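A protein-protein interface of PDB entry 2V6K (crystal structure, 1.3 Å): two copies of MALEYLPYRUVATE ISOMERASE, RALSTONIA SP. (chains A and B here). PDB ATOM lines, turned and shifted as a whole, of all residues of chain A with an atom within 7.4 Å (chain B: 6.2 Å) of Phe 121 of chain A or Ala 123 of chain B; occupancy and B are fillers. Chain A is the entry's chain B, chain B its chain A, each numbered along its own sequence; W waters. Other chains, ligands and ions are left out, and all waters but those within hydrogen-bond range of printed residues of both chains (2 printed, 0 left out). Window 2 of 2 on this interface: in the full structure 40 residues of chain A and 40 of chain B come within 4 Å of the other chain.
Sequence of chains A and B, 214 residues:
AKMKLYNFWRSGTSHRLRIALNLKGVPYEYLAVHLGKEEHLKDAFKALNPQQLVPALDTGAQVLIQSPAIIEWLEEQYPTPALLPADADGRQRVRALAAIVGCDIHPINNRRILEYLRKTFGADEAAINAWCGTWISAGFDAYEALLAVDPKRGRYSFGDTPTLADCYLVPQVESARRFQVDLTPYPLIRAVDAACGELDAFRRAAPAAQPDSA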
ATOM      1  N   ILE A 113     -12.310  27.917  -5.711  1.00  0.00           N
ATOM      2  CA  ILE A 113     -11.496  27.014  -4.901  1.00  0.00           C
ATOM      3  C   ILE A 113     -10.093  26.935  -5.489  1.00  0.00           C
ATOM      4  O   ILE A 113      -9.098  27.064  -4.768  1.00  0.00           O
ATOM      5  CB  ILE A 113     -12.119  25.599  -4.847  1.00  0.00           C
ATOM      6  CG1 ILE A 113     -13.600  25.648  -4.433  1.00  0.00           C
ATOM      7  CG2 ILE A 113     -11.309  24.690  -3.914  1.00  0.00           C
ATOM      8  CD1 ILE A 113     -13.877  26.289  -3.081  1.00  0.00           C
ATOM      9  N   GLU A 115      -8.668  29.094  -7.392  1.00  0.00           N
ATOM     10  CA  GLU A 115      -8.040  30.397  -7.163  1.00  0.00           C
ATOM     11  C   GLU A 115      -7.418  30.509  -5.780  1.00  0.00           C
ATOM     12  O   GLU A 115      -6.311  31.049  -5.627  1.00  0.00           O
ATOM     13  CB  GLU A 115      -9.042  31.518  -7.387  1.00  0.00           C
ATOM     14  CG  GLU A 115      -9.226  31.827  -8.852  1.00  0.00           C
ATOM     15  CD  GLU A 115      -7.931  32.316  -9.470  1.00  0.00           C
ATOM     16  OE1 GLU A 115      -7.519  33.450  -9.152  1.00  0.00           O
ATOM     17  OE2 GLU A 115      -7.304  31.561 -10.244  1.00  0.00           O
ATOM     18  N   TYR A 116      -8.121  29.994  -4.772  1.00  0.00           N
ATOM     19  CA  TYR A 116      -7.597  30.001  -3.415  1.00  0.00           C
ATOM     20  C   TYR A 116      -6.355  29.111  -3.321  1.00  0.00           C
ATOM     21  O   TYR A 116      -5.348  29.492  -2.711  1.00  0.00           O
ATOM     22  CB  TYR A 116      -8.685  29.538  -2.450  1.00  0.00           C
ATOM     23  CG  TYR A 116      -8.418  29.828  -0.989  1.00  0.00           C
ATOM     24  CD1 TYR A 116      -9.113  30.836  -0.324  1.00  0.00           C
ATOM     25  CD2 TYR A 116      -7.491  29.079  -0.265  1.00  0.00           C
ATOM     26  CE1 TYR A 116      -8.889  31.100   1.020  1.00  0.00           C
ATOM     27  CE2 TYR A 116      -7.261  29.335   1.078  1.00  0.00           C
ATOM     28  CZ  TYR A 116      -7.968  30.340   1.715  1.00  0.00           C
ATOM     29  OH  TYR A 116      -7.748  30.592   3.051  1.00  0.00           O
ATOM     30  N   LEU A 117      -6.402  27.938  -3.943  1.00  0.00           N
ATOM     31  CA  LEU A 117      -5.216  27.082  -3.972  1.00  0.00           C
ATOM     32  C   LEU A 117      -4.016  27.800  -4.587  1.00  0.00           C
ATOM     33  O   LEU A 117      -2.893  27.712  -4.074  1.00  0.00           O
ATOM     34  CB  LEU A 117      -5.495  25.786  -4.727  1.00  0.00           C
ATOM     35  CG  LEU A 117      -6.572  24.869  -4.155  1.00  0.00           C
ATOM     36  CD1 LEU A 117      -6.760  23.700  -5.084  1.00  0.00           C
ATOM     37  CD2 LEU A 117      -6.189  24.400  -2.753  1.00  0.00           C
ATOM     38  N   ARG A 118      -4.248  28.518  -5.680  1.00  0.00           N
ATOM     39  CA  ARG A 118      -3.170  29.250  -6.347  1.00  0.00           C
ATOM     40  C   ARG A 118      -2.628  30.378  -5.482  1.00  0.00           C
ATOM     41  O   ARG A 118      -1.412  30.506  -5.297  1.00  0.00           O
ATOM     42  CB  ARG A 118      -3.653  29.827  -7.677  1.00  0.00           C
ATOM     43  CG  ARG A 118      -3.957  28.788  -8.729  1.00  0.00           C
ATOM     44  CD  ARG A 118      -4.400  29.428 -10.042  1.00  0.00           C
ATOM     45  NE  ARG A 118      -4.793  28.392 -10.998  1.00  0.00           N
ATOM     46  CZ  ARG A 118      -6.046  28.120 -11.355  1.00  0.00           C
ATOM     47  NH1 ARG A 118      -7.059  28.827 -10.873  1.00  0.00           N
ATOM     48  NH2 ARG A 118      -6.288  27.139 -12.218  1.00  0.00           N
ATOM     49  N   LYS A 119      -3.529  31.194  -4.956  1.00  0.00           N
ATOM     50  CA  LYS A 119      -3.151  32.455  -4.332  1.00  0.00           C
ATOM     51  C   LYS A 119      -2.756  32.323  -2.873  1.00  0.00           C
ATOM     52  O   LYS A 119      -1.949  33.117  -2.385  1.00  0.00           O
ATOM     53  CB  LYS A 119      -4.257  33.496  -4.526  1.00  0.00           C
ATOM     54  CG  LYS A 119      -4.359  33.920  -5.987  1.00  0.00           C
ATOM     55  CD  LYS A 119      -5.443  34.935  -6.260  1.00  0.00           C
ATOM     56  CE  LYS A 119      -5.210  35.572  -7.628  1.00  0.00           C
ATOM     57  NZ  LYS A 119      -4.978  34.558  -8.713  1.00  0.00           N
ATOM     58  N   THR A 120      -3.302  31.322  -2.188  1.00  0.00           N
ATOM     59  CA  THR A 120      -2.987  31.100  -0.779  1.00  0.00           C
ATOM     60  C   THR A 120      -1.973  29.973  -0.600  1.00  0.00           C
ATOM     61  O   THR A 120      -1.053  30.093   0.216  1.00  0.00           O
ATOM     62  CB  THR A 120      -4.265  30.870   0.054  1.00  0.00           C
ATOM     63  OG1 THR A 120      -5.078  32.046  -0.029  1.00  0.00           O
ATOM     64  CG2 THR A 120      -3.935  30.602   1.520  1.00  0.00           C
ATOM     65  N   PHE A 121      -2.115  28.899  -1.369  1.00  0.00           N
ATOM     66  CA  PHE A 121      -1.225  27.752  -1.206  1.00  0.00           C
ATOM     67  C   PHE A 121      -0.151  27.635  -2.283  1.00  0.00           C
ATOM     68  O   PHE A 121       0.670  26.718  -2.241  1.00  0.00           O
ATOM     69  CB  PHE A 121      -2.037  26.463  -1.065  1.00  0.00           C
ATOM     70  CG  PHE A 121      -2.834  26.402   0.205  1.00  0.00           C
ATOM     71  CD1 PHE A 121      -2.186  26.406   1.439  1.00  0.00           C
ATOM     72  CD2 PHE A 121      -4.221  26.363   0.173  1.00  0.00           C
ATOM     73  CE1 PHE A 121      -2.913  26.366   2.622  1.00  0.00           C
ATOM     74  CE2 PHE A 121      -4.956  26.316   1.355  1.00  0.00           C
ATOM     75  CZ  PHE A 121      -4.302  26.319   2.579  1.00  0.00           C
ATOM     76  N   GLY A 122      -0.141  28.579  -3.223  1.00  0.00           N
ATOM     77  CA  GLY A 122       0.908  28.646  -4.242  1.00  0.00           C
ATOM     78  C   GLY A 122       0.876  27.522  -5.257  1.00  0.00           C
ATOM     79  O   GLY A 122       1.892  27.242  -5.907  1.00  0.00           O
ATOM     80  N   ALA A 123      -0.285  26.883  -5.415  1.00  0.00           N
ATOM     81  CA  ALA A 123      -0.428  25.758  -6.332  1.00  0.00           C
ATOM     82  C   ALA A 123      -0.091  26.152  -7.764  1.00  0.00           C
ATOM     83  O   ALA A 123      -0.604  27.155  -8.280  1.00  0.00           O
ATOM     84  CB  ALA A 123      -1.851  25.208  -6.263  1.00  0.00           C
ATOM     85  N   ASP A 124       0.767  25.368  -8.413  1.00  0.00           N
ATOM     86  CA  ASP A 124       0.956  25.533  -9.846  1.00  0.00           C
ATOM     87  C   ASP A 124      -0.069  24.685 -10.590  1.00  0.00           C
ATOM     88  O   ASP A 124      -0.888  24.005  -9.962  1.00  0.00           O
ATOM     89  CB  ASP A 124       2.404  25.257 -10.280  1.00  0.00           C
ATOM     90  CG  ASP A 124       2.830  23.799 -10.128  1.00  0.00           C
ATOM     91  OD1 ASP A 124       2.020  22.908  -9.811  1.00  0.00           O
ATOM     92  OD2 ASP A 124       4.036  23.546 -10.352  1.00  0.00           O
ATOM     93  N   ALA A 127      -0.308  20.989  -9.832  1.00  0.00           N
ATOM     94  CA  ALA A 127      -0.950  20.765  -8.538  1.00  0.00           C
ATOM     95  C   ALA A 127      -2.463  20.943  -8.633  1.00  0.00           C
ATOM     96  O   ALA A 127      -3.217  20.182  -8.021  1.00  0.00           O
ATOM     97  CB  ALA A 127      -0.367  21.685  -7.472  1.00  0.00           C
ATOM     98  N   TRP A 131      -5.170  17.964  -7.832  1.00  0.00           N
ATOM     99  CA  TRP A 131      -6.310  18.204  -6.935  1.00  0.00           C
ATOM    100  C   TRP A 131      -7.607  17.797  -7.621  1.00  0.00           C
ATOM    101  O   TRP A 131      -8.364  16.970  -7.106  1.00  0.00           O
ATOM    102  CB  TRP A 131      -6.340  19.686  -6.573  1.00  0.00           C
ATOM    103  CG  TRP A 131      -7.582  20.226  -5.907  1.00  0.00           C
ATOM    104  CD1 TRP A 131      -8.718  20.672  -6.522  1.00  0.00           C
ATOM    105  CD2 TRP A 131      -7.773  20.440  -4.505  1.00  0.00           C
ATOM    106  NE1 TRP A 131      -9.614  21.135  -5.581  1.00  0.00           N
ATOM    107  CE2 TRP A 131      -9.052  21.015  -4.338  1.00  0.00           C
ATOM    108  CE3 TRP A 131      -6.978  20.217  -3.371  1.00  0.00           C
ATOM    109  CZ2 TRP A 131      -9.558  21.361  -3.082  1.00  0.00           C
ATOM    110  CZ3 TRP A 131      -7.480  20.555  -2.131  1.00  0.00           C
ATOM    111  CH2 TRP A 131      -8.758  21.121  -1.995  1.00  0.00           C
ATOM    112  N   LEU B 114      -9.448  18.765   3.990  1.00  0.00           N
ATOM    113  CA  LEU B 114      -8.492  19.354   4.921  1.00  0.00           C
ATOM    114  C   LEU B 114      -7.226  18.518   5.018  1.00  0.00           C
ATOM    115  O   LEU B 114      -6.121  19.064   5.104  1.00  0.00           O
ATOM    116  CB  LEU B 114      -9.139  19.549   6.294  1.00  0.00           C
ATOM    117  CG  LEU B 114     -10.468  20.323   6.289  1.00  0.00           C
ATOM    118  CD1 LEU B 114     -10.919  20.588   7.722  1.00  0.00           C
ATOM    119  CD2 LEU B 114     -10.382  21.630   5.519  1.00  0.00           C
ATOM    120  N   LEU B 117      -5.137  19.404   2.041  1.00  0.00           N
ATOM    121  CA  LEU B 117      -4.470  20.686   2.293  1.00  0.00           C
ATOM    122  C   LEU B 117      -3.251  20.521   3.190  1.00  0.00           C
ATOM    123  O   LEU B 117      -2.198  21.108   2.927  1.00  0.00           O
ATOM    124  CB  LEU B 117      -5.443  21.695   2.894  1.00  0.00           C
ATOM    125  CG  LEU B 117      -6.645  22.097   2.035  1.00  0.00           C
ATOM    126  CD1 LEU B 117      -7.530  23.033   2.812  1.00  0.00           C
ATOM    127  CD2 LEU B 117      -6.195  22.748   0.734  1.00  0.00           C
ATOM    128  N   ARG B 118      -3.387  19.727   4.247  1.00  0.00           N
ATOM    129  CA  ARG B 118      -2.278  19.489   5.169  1.00  0.00           C
ATOM    130  C   ARG B 118      -1.128  18.742   4.505  1.00  0.00           C
ATOM    131  O   ARG B 118       0.027  19.155   4.598  1.00  0.00           O
ATOM    132  CB  ARG B 118      -2.758  18.689   6.381  1.00  0.00           C
ATOM    133  CG  ARG B 118      -3.724  19.437   7.280  1.00  0.00           C
ATOM    134  CD  ARG B 118      -4.168  18.586   8.464  1.00  0.00           C
ATOM    135  NE  ARG B 118      -5.160  19.307   9.264  1.00  0.00           N
ATOM    136  CZ  ARG B 118      -6.448  18.984   9.354  1.00  0.00           C
ATOM    137  NH1 ARG B 118      -6.937  17.927   8.715  1.00  0.00           N
ATOM    138  NH2 ARG B 118      -7.258  19.729  10.100  1.00  0.00           N
ATOM    139  N   LYS B 119      -1.446  17.645   3.830  1.00  0.00           N
ATOM    140  CA  LYS B 119      -0.420  16.712   3.369  1.00  0.00           C
ATOM    141  C   LYS B 119       0.180  17.071   2.023  1.00  0.00           C
ATOM    142  O   LYS B 119       1.331  16.731   1.754  1.00  0.00           O
ATOM    143  CB  LYS B 119      -0.968  15.282   3.387  1.00  0.00           C
ATOM    144  CG  LYS B 119      -1.257  14.829   4.816  1.00  0.00           C
ATOM    145  CD  LYS B 119      -1.790  13.419   4.921  1.00  0.00           C
ATOM    146  CE  LYS B 119      -1.610  12.909   6.348  1.00  0.00           C
ATOM    147  NZ  LYS B 119      -2.111  13.876   7.388  1.00  0.00           N
ATOM    148  N   THR B 120      -0.588  17.773   1.193  1.00  0.00           N
ATOM    149  CA  THR B 120      -0.108  18.184  -0.129  1.00  0.00           C
ATOM    150  C   THR B 120       0.342  19.640  -0.147  1.00  0.00           C
ATOM    151  O   THR B 120       1.374  19.957  -0.745  1.00  0.00           O
ATOM    152  CB  THR B 120      -1.157  17.891  -1.223  1.00  0.00           C
ATOM    153  OG1 THR B 120      -1.395  16.480  -1.259  1.00  0.00           O
ATOM    154  CG2 THR B 120      -0.669  18.342  -2.600  1.00  0.00           C
ATOM    155  N   PHE B 121      -0.411  20.515   0.515  1.00  0.00           N
ATOM    156  CA  PHE B 121      -0.086  21.941   0.510  1.00  0.00           C
ATOM    157  C   PHE B 121       0.557  22.434   1.805  1.00  0.00           C
ATOM    158  O   PHE B 121       0.887  23.619   1.923  1.00  0.00           O
ATOM    159  CB  PHE B 121      -1.315  22.768   0.126  1.00  0.00           C
ATOM    160  CG  PHE B 121      -1.764  22.534  -1.283  1.00  0.00           C
ATOM    161  CD1 PHE B 121      -0.926  22.858  -2.346  1.00  0.00           C
ATOM    162  CD2 PHE B 121      -3.003  21.971  -1.551  1.00  0.00           C
ATOM    163  CE1 PHE B 121      -1.323  22.634  -3.656  1.00  0.00           C
ATOM    164  CE2 PHE B 121      -3.411  21.746  -2.861  1.00  0.00           C
ATOM    165  CZ  PHE B 121      -2.570  22.077  -3.915  1.00  0.00           C
ATOM    166  N   GLY B 122       0.758  21.525   2.756  1.00  0.00           N
ATOM    167  CA  GLY B 122       1.472  21.851   3.992  1.00  0.00           C
ATOM    168  C   GLY B 122       0.743  22.816   4.906  1.00  0.00           C
ATOM    169  O   GLY B 122       1.369  23.493   5.727  1.00  0.00           O
ATOM    170  N   ALA B 123      -0.584  22.874   4.785  1.00  0.00           N
ATOM    171  CA  ALA B 123      -1.390  23.789   5.583  1.00  0.00           C
ATOM    172  C   ALA B 123      -1.237  23.515   7.073  1.00  0.00           C
ATOM    173  O   ALA B 123      -1.366  22.365   7.518  1.00  0.00           O
ATOM    174  CB  ALA B 123      -2.858  23.679   5.177  1.00  0.00           C
ATOM    175  N   ASP B 124      -0.966  24.564   7.845  1.00  0.00           N
ATOM    176  CA  ASP B 124      -1.045  24.438   9.293  1.00  0.00           C
ATOM    177  C   ASP B 124      -2.472  24.735   9.741  1.00  0.00           C
ATOM    178  O   ASP B 124      -3.339  25.032   8.911  1.00  0.00           O
ATOM    179  CB  ASP B 124       0.018  25.282  10.021  1.00  0.00           C
ATOM    180  CG  ASP B 124      -0.163  26.785   9.855  1.00  0.00           C
ATOM    181  OD1 ASP B 124      -1.203  27.265   9.360  1.00  0.00           O
ATOM    182  OD2 ASP B 124       0.774  27.509  10.255  1.00  0.00           O
ATOM    183  N   GLU B 125      -2.738  24.637  11.035  1.00  0.00           N
ATOM    184  CA  GLU B 125      -4.121  24.724  11.481  1.00  0.00           C
ATOM    185  C   GLU B 125      -4.717  26.116  11.346  1.00  0.00           C
ATOM    186  O   GLU B 125      -5.918  26.247  11.128  1.00  0.00           O
ATOM    187  CB  GLU B 125      -4.303  24.145  12.886  1.00  0.00           C
ATOM    188  CG  GLU B 125      -4.079  22.623  12.952  1.00  0.00           C
ATOM    189  CD  GLU B 125      -4.797  21.850  11.845  1.00  0.00           C
ATOM    190  OE1 GLU B 125      -6.034  21.966  11.721  1.00  0.00           O
ATOM    191  OE2 GLU B 125      -4.119  21.109  11.101  1.00  0.00           O
ATOM    192  N   ALA B 127      -4.054  27.990   8.777  1.00  0.00           N
ATOM    193  CA  ALA B 127      -4.426  27.980   7.362  1.00  0.00           C
ATOM    194  C   ALA B 127      -5.705  27.180   7.122  1.00  0.00           C
ATOM    195  O   ALA B 127      -6.541  27.575   6.307  1.00  0.00           O
ATOM    196  CB  ALA B 127      -3.291  27.434   6.513  1.00  0.00           C
ATOM    197  N   ILE B 128      -5.858  26.066   7.839  1.00  0.00           N
ATOM    198  CA  ILE B 128      -7.085  25.267   7.774  1.00  0.00           C
ATOM    199  C   ILE B 128      -8.278  26.095   8.236  1.00  0.00           C
ATOM    200  O   ILE B 128      -9.302  26.136   7.554  1.00  0.00           O
ATOM    201  CB  ILE B 128      -6.960  23.954   8.592  1.00  0.00           C
ATOM    202  CG1 ILE B 128      -5.917  23.005   7.972  1.00  0.00           C
ATOM    203  CG2 ILE B 128      -8.323  23.266   8.759  1.00  0.00           C
ATOM    204  CD1 ILE B 128      -6.216  22.554   6.542  1.00  0.00           C
ATOM    205  N   TRP B 131      -9.187  28.736   5.590  1.00  0.00           N
ATOM    206  CA  TRP B 131      -9.880  28.076   4.486  1.00  0.00           C
ATOM    207  C   TRP B 131     -11.341  27.855   4.846  1.00  0.00           C
ATOM    208  O   TRP B 131     -12.241  28.297   4.126  1.00  0.00           O
ATOM    209  CB  TRP B 131      -9.187  26.746   4.195  1.00  0.00           C
ATOM    210  CG  TRP B 131      -9.908  25.755   3.299  1.00  0.00           C
ATOM    211  CD1 TRP B 131     -10.839  24.828   3.676  1.00  0.00           C
ATOM    212  CD2 TRP B 131      -9.686  25.550   1.898  1.00  0.00           C
ATOM    213  NE1 TRP B 131     -11.233  24.079   2.588  1.00  0.00           N
ATOM    214  CE2 TRP B 131     -10.525  24.487   1.488  1.00  0.00           C
ATOM    215  CE3 TRP B 131      -8.853  26.157   0.947  1.00  0.00           C
ATOM    216  CZ2 TRP B 131     -10.560  24.028   0.171  1.00  0.00           C
ATOM    217  CZ3 TRP B 131      -8.883  25.699  -0.355  1.00  0.00           C
ATOM    218  CH2 TRP B 131      -9.730  24.646  -0.733  1.00  0.00           C
HETATM  219  O   HOH W   1       1.623  25.485  -0.028  1.00  0.00           O
HETATM  220  O   HOH W   2      -5.849  29.180   4.188  1.00  0.00           O
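Of the printed residues of chain B, Ile 113 of chain A touches Trp 131. Printed residues of chain B within 4 Å of Tyr 116 of chain A: Trp 131 (3.4 Å). Of the printed residues of chain B, Leu 117 of chain A touches Leu 117 (3.9 Å), Phe 121 (3.8 Å) and Trp 131 (3.8 Å). Of chain B, only Leu 117, Phe 121, Ala 123 and Trp 131 come within 4 Å of Phe 121 of chain A. No residue of chain A comes within 4 Å of Gly 122 of chain B. Ala 123 of chain B touches just one residue of chain A: Phe 121. Of the printed residues of chain A, Trp 131 of chain B touches Ile 113 (3.6 Å), Tyr 116 (3.4 Å), Leu 117 (3.8 Å), Phe 121 (3.9 Å) and Trp 131 (3.9 Å). The nearest residue of chain B that does not touch Phe 121 of chain A is Ala 127 of chain B (4.1 Å).
Of the 13 printed residues of chain A, 6 touch a printed residue of chain B. Printed residues of chain A that touch a printed residue of chain B: Ile 113, Tyr 116, Leu 117, Phe 121, Ala 123 and Trp 131. Hydrophobic or aromatic side chains of chain A that line the printed part of chain B: Ile 113, Tyr 116, Leu 117, Phe 121, Ala 123 and Trp 131. Of the 13 printed residues of chain B, 4 touch a printed residue of chain A. Among the printed residues, 13 pairs touch across the chains. Among the printed residues, no Asp or Glu carboxylate lies within 4 Å of a Lys or Arg side-chain nitrogen of the other chain.
N of Trp 131 of chain B is in hydrogen-bond range of OH of Tyr 116 of chain A (3.5 Å).
Among the printed residues, merely in contact across the chains: Ile 113 of chain A with Trp 131 of chain B, Ala 123 of chain A with Phe 121 of chain B, Phe 121 of chain A with Ala 123 of chain B, Phe 121 of chain A with Leu 117 of chain B, Trp 131 of chain A with Leu 117 of chain B, Leu 117 of chain A with Trp 131 of chain B, Leu 117 of chain A with Phe 121 of chain B, Leu 117 of chain A with Leu 117 of chain B, Trp 131 of chain A with Trp 131 of chain B, Trp 131 of chain A with Phe 121 of chain B, Phe 121 of chain A with Trp 131 of chain B and Phe 121 of chain A with Phe 121 of chain B.
Leu 117 of chain B touches its own counterpart, Leu 117 of chain A. Leu 117 of chain A touches Phe 121 of chain B, and with the chains exchanged Phe 121 of chain A touches Leu 117 of chain B. Leu 117 of chain A touches Trp 131 of chain B, and with the chains exchanged Trp 131 of chain A touches Leu 117 of chain B. Phe 121 of chain A touches Trp 131 of chain B, and with the chains exchanged Trp 131 of chain A touches Phe 121 of chain B. Of the 13 pairs that touch across the chains among the printed residues, 11 have their exchanged pair printed and touching as well.
Water W2 bridges the side-chain hydroxyl (OH) of Tyr 116 of chain A (2.6 Å) and the backbone carbonyl oxygen (O) of Ala 127 of chain B (2.7 Å). Water W1 lies within hydrogen-bond range of the backbone carbonyl oxygen (O) of Phe 121 of chain A (2.7 Å) and the backbone carbonyl oxygen (O) of Phe 121 of chain B (2.8 Å).
N of Ala 123 of chain A sits at hydrogen-bond distance from O of Leu 117 of chain A (3.0 Å). N of Ala 123 of chain B is in hydrogen-bond range of O of Leu 117 of chain B (3.0 Å). The backbone carbonyl oxygen of Leu 117 of chain B lies within hydrogen-bond range of the backbone NH of Gly 122 of chain B, 3.0 Å away. The backbone carbonyl oxygen of Leu 117 of chain A sits at hydrogen-bond distance from the backbone NH of Gly 122 of chain A (3.0 Å).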
